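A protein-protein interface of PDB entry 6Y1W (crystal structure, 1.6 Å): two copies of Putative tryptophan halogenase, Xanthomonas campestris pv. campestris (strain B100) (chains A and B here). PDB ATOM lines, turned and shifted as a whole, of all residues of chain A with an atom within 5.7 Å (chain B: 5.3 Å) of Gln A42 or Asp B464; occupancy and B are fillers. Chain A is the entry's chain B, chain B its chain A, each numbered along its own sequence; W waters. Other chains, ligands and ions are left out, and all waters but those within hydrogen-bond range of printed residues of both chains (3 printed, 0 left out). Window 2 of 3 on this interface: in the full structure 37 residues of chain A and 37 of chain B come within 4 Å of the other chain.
Among the printed residues, pairs that only touch across the chains: Gln A42 with Leu B465, Gln A42 with Asp B464, Arg A41 with Leu B465, Gln A367 with Pro B461 and Leu A39 with Val B462.
Gln A42 touches just these residues of chain B: Pro B461 (2.8 Å), Asp B464 (3.7 Å) and Leu B465 (3.4 Å). Asp B464 touches two residues of chain A. Of the printed residues of chain B, Leu A39 touches Val B462 (3.8 Å). Of the printed residues of chain B, Arg A41 touches Leu B465. The nearest printed residue of chain A that does not touch Asp B464 is Leu A39 (7.0 Å).
No position is printed for both chains. Of the 8 pairs that touch across the chains among the printed residues, none has its exchanged pair printed and touching as well.
NZ of Lys B126 is in salt-bridge range of OD1 of Asp B464 (2.8 Å). A ring nitrogen (NE2) of His B459 sits at hydrogen-bond distance from the side-chain carboxylate (OD1) of Asp B464 (3.0 Å). A ring nitrogen (ND1) of His B460 lies within hydrogen-bond range of the backbone NH of Val B462, 3.0 Å away.
Of the 8 printed residues of chain A, 4 touch a printed residue of chain B. Hydrophobic or aromatic side chains of chain A within 4 Å of the printed part of chain B: Leu A39. Of the 9 printed residues of chain B, 5 touch a printed residue of chain A. Hydrophobic or aromatic side chains of chain B that line the printed part of chain A: His B459, Pro B461 and Leu B465. Among the printed residues, no Asp or Glu carboxylate lies within 4 Å of a Lys or Arg side-chain nitrogen of the other chain.
Water W1 lies within hydrogen-bond range of O of Leu B465 (2.4 Å) and NH1 of Arg A41 (3.2 Å). Water W2 bridges OD1 of Asp B464 and NE2 of Gln A367. Water W3 bridges the side-chain amide oxygen of Gln A42 and the backbone carbonyl oxygen of Asp B464.
N of His B459 sits at hydrogen-bond distance from OE1 of Gln A367 (3.1 Å). The backbone carbonyl oxygen (O) of Pro B461 is in hydrogen-bond range of the side-chain amide nitrogen (NE2) of Gln A42, 2.8 Å away. NE2 of Gln A367 sits at hydrogen-bond distance from OD2 of Asp B464, 2.9 Å away.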
ATOM      1  N   ARG A  17     -23.677  -1.134  -0.749  1.00  0.00           N
ATOM      2  CA  ARG A  17     -25.119  -0.989  -0.710  1.00  0.00           C
ATOM      3  C   ARG A  17     -25.692  -0.320  -1.941  1.00  0.00           C
ATOM      4  O   ARG A  17     -26.880  -0.515  -2.236  1.00  0.00           O
ATOM      5  CB  ARG A  17     -25.559  -0.160   0.516  1.00  0.00           C
ATOM      6  CG  ARG A  17     -25.226  -0.843   1.838  1.00  0.00           C
ATOM      7  CD  ARG A  17     -25.767  -0.050   3.013  1.00  0.00           C
ATOM      8  NE  ARG A  17     -24.702   0.396   3.909  1.00  0.00           N
ATOM      9  CZ  ARG A  17     -24.591   0.022   5.182  1.00  0.00           C
ATOM     10  NH1 ARG A  17     -25.483  -0.805   5.716  1.00  0.00           N
ATOM     11  NH2 ARG A  17     -23.587   0.476   5.922  1.00  0.00           N
ATOM     12  N   LEU A  39     -30.388  -9.404  -6.263  1.00  0.00           N
ATOM     13  CA  LEU A  39     -30.052  -8.667  -5.047  1.00  0.00           C
ATOM     14  C   LEU A  39     -30.820  -7.363  -4.888  1.00  0.00           C
ATOM     15  O   LEU A  39     -30.539  -6.620  -3.947  1.00  0.00           O
ATOM     16  CB  LEU A  39     -28.547  -8.384  -5.015  1.00  0.00           C
ATOM     17  CG  LEU A  39     -27.643  -9.600  -4.921  1.00  0.00           C
ATOM     18  CD1 LEU A  39     -26.171  -9.230  -5.095  1.00  0.00           C
ATOM     19  CD2 LEU A  39     -27.872 -10.294  -3.565  1.00  0.00           C
ATOM     20  N   GLY A  40     -31.787  -7.094  -5.752  1.00  0.00           N
ATOM     21  CA  GLY A  40     -32.470  -5.810  -5.763  1.00  0.00           C
ATOM     22  C   GLY A  40     -33.265  -5.504  -4.511  1.00  0.00           C
ATOM     23  O   GLY A  40     -33.607  -4.325  -4.275  1.00  0.00           O
ATOM     24  N   ARG A  41     -33.574  -6.522  -3.701  1.00  0.00           N
ATOM     25  CA  ARG A  41     -34.307  -6.247  -2.463  1.00  0.00           C
ATOM     26  C   ARG A  41     -33.439  -5.596  -1.400  1.00  0.00           C
ATOM     27  O   ARG A  41     -33.987  -5.027  -0.442  1.00  0.00           O
ATOM     28  CB  ARG A  41     -34.924  -7.531  -1.913  1.00  0.00           C
ATOM     29  CG  ARG A  41     -36.176  -7.959  -2.661  1.00  0.00           C
ATOM     30  CD  ARG A  41     -36.776  -9.245  -2.084  1.00  0.00           C
ATOM     31  NE  ARG A  41     -36.044 -10.425  -2.521  1.00  0.00           N
ATOM     32  CZ  ARG A  41     -35.859 -11.512  -1.773  1.00  0.00           C
ATOM     33  NH1 ARG A  41     -36.351 -11.565  -0.540  1.00  0.00           N
ATOM     34  NH2 ARG A  41     -35.179 -12.542  -2.259  1.00  0.00           N
ATOM     35  N   GLN A  42     -32.115  -5.703  -1.501  1.00  0.00           N
ATOM     36  CA  GLN A  42     -31.219  -5.069  -0.538  1.00  0.00           C
ATOM     37  C   GLN A  42     -30.232  -4.071  -1.120  1.00  0.00           C
ATOM     38  O   GLN A  42     -29.467  -3.482  -0.354  1.00  0.00           O
ATOM     39  CB  GLN A  42     -30.439  -6.119   0.259  1.00  0.00           C
ATOM     40  CG  GLN A  42     -29.389  -6.867  -0.530  1.00  0.00           C
ATOM     41  CD  GLN A  42     -28.963  -8.116   0.235  1.00  0.00           C
ATOM     42  OE1 GLN A  42     -29.592  -8.481   1.242  1.00  0.00           O
ATOM     43  NE2 GLN A  42     -27.920  -8.772  -0.233  1.00  0.00           N
ATOM     44  N   LEU A  43     -30.144  -3.942  -2.438  1.00  0.00           N
ATOM     45  CA  LEU A  43     -29.210  -3.025  -3.086  1.00  0.00           C
ATOM     46  C   LEU A  43     -29.992  -1.907  -3.737  1.00  0.00           C
ATOM     47  O   LEU A  43     -31.095  -2.124  -4.238  1.00  0.00           O
ATOM     48  CB  LEU A  43     -28.393  -3.709  -4.203  1.00  0.00           C
ATOM     49  CG  LEU A  43     -27.215  -4.604  -3.909  1.00  0.00           C
ATOM     50  CD1 LEU A  43     -26.722  -5.110  -5.267  1.00  0.00           C
ATOM     51  CD2 LEU A  43     -26.105  -3.868  -3.172  1.00  0.00           C
ATOM     52  N   GLN A  44     -29.425  -0.706  -3.711  1.00  0.00           N
ATOM     53  CA  GLN A  44     -29.934   0.409  -4.482  1.00  0.00           C
ATOM     54  C   GLN A  44     -29.159   0.406  -5.797  1.00  0.00           C
ATOM     55  O   GLN A  44     -27.936   0.546  -5.786  1.00  0.00           O
ATOM     56  CB  GLN A  44     -29.748   1.722  -3.727  1.00  0.00           C
ATOM     57  CG  GLN A  44     -30.332   2.937  -4.456  1.00  0.00           C
ATOM     58  CD  GLN A  44     -30.026   4.231  -3.743  1.00  0.00           C
ATOM     59  OE1 GLN A  44     -29.527   4.228  -2.613  1.00  0.00           O
ATOM     60  NE2 GLN A  44     -30.320   5.356  -4.399  1.00  0.00           N
ATOM     61  N   GLN A 367     -19.760  -8.335  -0.216  1.00  0.00           N
ATOM     62  CA  GLN A 367     -20.235  -7.676   0.999  1.00  0.00           C
ATOM     63  C   GLN A 367     -19.406  -6.424   1.219  1.00  0.00           C
ATOM     64  O   GLN A 367     -19.929  -5.311   1.354  1.00  0.00           O
ATOM     65  CB  GLN A 367     -20.109  -8.638   2.204  1.00  0.00           C
ATOM     66  CG  GLN A 367     -21.390  -8.840   3.012  1.00  0.00           C
ATOM     67  CD  GLN A 367     -21.273  -9.948   4.071  1.00  0.00           C
ATOM     68  OE1 GLN A 367     -20.167 -10.333   4.496  1.00  0.00           O
ATOM     69  NE2 GLN A 367     -22.410 -10.464   4.492  1.00  0.00           N
ATOM     70  N   LYS B 126     -23.749 -17.332   7.334  1.00  0.00           N
ATOM     71  CA  LYS B 126     -24.744 -16.385   7.828  1.00  0.00           C
ATOM     72  C   LYS B 126     -25.492 -17.005   8.989  1.00  0.00           C
ATOM     73  O   LYS B 126     -25.703 -16.362  10.029  1.00  0.00           O
ATOM     74  CB  LYS B 126     -25.703 -16.011   6.702  1.00  0.00           C
ATOM     75  CG  LYS B 126     -26.954 -15.262   7.125  1.00  0.00           C
ATOM     76  CD  LYS B 126     -26.730 -13.807   7.241  1.00  0.00           C
ATOM     77  CE  LYS B 126     -28.062 -13.111   7.474  1.00  0.00           C
ATOM     78  NZ  LYS B 126     -27.679 -11.693   7.673  1.00  0.00           N
ATOM     79  N   HIS B 459     -19.278 -13.317   4.144  1.00  0.00           N
ATOM     80  CA  HIS B 459     -19.931 -14.305   3.294  1.00  0.00           C
ATOM     81  C   HIS B 459     -20.666 -13.591   2.169  1.00  0.00           C
ATOM     82  O   HIS B 459     -20.799 -12.359   2.160  1.00  0.00           O
ATOM     83  CB  HIS B 459     -20.908 -15.163   4.098  1.00  0.00           C
ATOM     84  CG  HIS B 459     -22.006 -14.370   4.732  1.00  0.00           C
ATOM     85  ND1 HIS B 459     -22.012 -14.043   6.072  1.00  0.00           N
ATOM     86  CD2 HIS B 459     -23.140 -13.847   4.211  1.00  0.00           C
ATOM     87  CE1 HIS B 459     -23.096 -13.339   6.343  1.00  0.00           C
ATOM     88  NE2 HIS B 459     -23.790 -13.195   5.232  1.00  0.00           N
ATOM     89  N   HIS B 460     -21.173 -14.387   1.226  1.00  0.00           N
ATOM     90  CA  HIS B 460     -21.863 -13.820   0.073  1.00  0.00           C
ATOM     91  C   HIS B 460     -23.100 -13.062   0.545  1.00  0.00           C
ATOM     92  O   HIS B 460     -23.907 -13.603   1.312  1.00  0.00           O
ATOM     93  CB  HIS B 460     -22.249 -14.936  -0.902  1.00  0.00           C
ATOM     94  CG  HIS B 460     -22.629 -14.455  -2.265  1.00  0.00           C
ATOM     95  ND1 HIS B 460     -23.692 -13.616  -2.481  1.00  0.00           N
ATOM     96  CD2 HIS B 460     -22.102 -14.722  -3.491  1.00  0.00           C
ATOM     97  CE1 HIS B 460     -23.818 -13.377  -3.777  1.00  0.00           C
ATOM     98  NE2 HIS B 460     -22.864 -14.037  -4.410  1.00  0.00           N
ATOM     99  N   PRO B 461     -23.286 -11.810   0.121  1.00  0.00           N
ATOM    100  CA  PRO B 461     -24.465 -11.048   0.574  1.00  0.00           C
ATOM    101  C   PRO B 461     -25.819 -11.623   0.147  1.00  0.00           C
ATOM    102  O   PRO B 461     -26.845 -11.203   0.696  1.00  0.00           O
ATOM    103  CB  PRO B 461     -24.235  -9.643  -0.012  1.00  0.00           C
ATOM    104  CG  PRO B 461     -23.254  -9.825  -1.103  1.00  0.00           C
ATOM    105  CD  PRO B 461     -22.395 -11.019  -0.758  1.00  0.00           C
ATOM    106  N   VAL B 462     -25.884 -12.574  -0.787  1.00  0.00           N
ATOM    107  CA  VAL B 462     -27.194 -13.118  -1.107  1.00  0.00           C
ATOM    108  C   VAL B 462     -27.799 -13.793   0.135  1.00  0.00           C
ATOM    109  O   VAL B 462     -29.020 -13.840   0.284  1.00  0.00           O
ATOM    110  CB  VAL B 462     -27.117 -14.092  -2.297  1.00  0.00           C
ATOM    111  CG1 VAL B 462     -26.511 -15.421  -1.862  1.00  0.00           C
ATOM    112  CG2 VAL B 462     -28.495 -14.310  -2.893  1.00  0.00           C
ATOM    113  N   ALA B 463     -26.956 -14.278   1.041  1.00  0.00           N
ATOM    114  CA  ALA B 463     -27.511 -14.911   2.236  1.00  0.00           C
ATOM    115  C   ALA B 463     -28.116 -13.864   3.166  1.00  0.00           C
ATOM    116  O   ALA B 463     -28.949 -14.198   4.019  1.00  0.00           O
ATOM    117  CB  ALA B 463     -26.425 -15.720   2.933  1.00  0.00           C
ATOM    118  N   ASP B 464     -27.762 -12.593   3.002  1.00  0.00           N
ATOM    119  CA  ASP B 464     -28.348 -11.596   3.904  1.00  0.00           C
ATOM    120  C   ASP B 464     -29.800 -11.305   3.557  1.00  0.00           C
ATOM    121  O   ASP B 464     -30.478 -10.590   4.313  1.00  0.00           O
ATOM    122  CB  ASP B 464     -27.537 -10.293   3.882  1.00  0.00           C
ATOM    123  CG  ASP B 464     -26.151 -10.451   4.458  1.00  0.00           C
ATOM    124  OD1 ASP B 464     -25.983 -11.104   5.523  1.00  0.00           O
ATOM    125  OD2 ASP B 464     -25.209  -9.909   3.862  1.00  0.00           O
ATOM    126  N   LEU B 465     -30.300 -11.856   2.449  1.00  0.00           N
ATOM    127  CA  LEU B 465     -31.695 -11.714   2.087  1.00  0.00           C
ATOM    128  C   LEU B 465     -32.593 -12.553   2.992  1.00  0.00           C
ATOM    129  O   LEU B 465     -33.802 -12.309   3.047  1.00  0.00           O
ATOM    130  CB  LEU B 465     -31.919 -12.136   0.634  1.00  0.00           C
ATOM    131  CG  LEU B 465     -31.395 -11.181  -0.460  1.00  0.00           C
ATOM    132  CD1 LEU B 465     -31.518 -11.857  -1.816  1.00  0.00           C
ATOM    133  CD2 LEU B 465     -32.160  -9.885  -0.454  1.00  0.00           C
ATOM    134  N   MET B 466     -32.049 -13.581   3.645  1.00  0.00           N
ATOM    135  CA  MET B 466     -32.877 -14.472   4.445  1.00  0.00           C
ATOM    136  C   MET B 466     -32.944 -14.040   5.901  1.00  0.00           C
ATOM    137  O   MET B 466     -31.914 -13.878   6.559  1.00  0.00           O
ATOM    138  CB  MET B 466     -32.357 -15.899   4.347  1.00  0.00           C
ATOM    139  CG  MET B 466     -32.472 -16.411   2.929  1.00  0.00           C
ATOM    140  SD  MET B 466     -31.584 -17.949   2.834  1.00  0.00           S
ATOM    141  CE  MET B 466     -32.878 -19.047   3.217  1.00  0.00           C
HETATM  142  O   HOH W   1     -35.381 -13.569   1.689  1.00  0.00           O
HETATM  143  O   HOH W   2     -24.392  -9.875   7.105  1.00  0.00           O
HETATM  144  O   HOH W   3     -31.288  -8.090   3.193  1.00  0.00           O
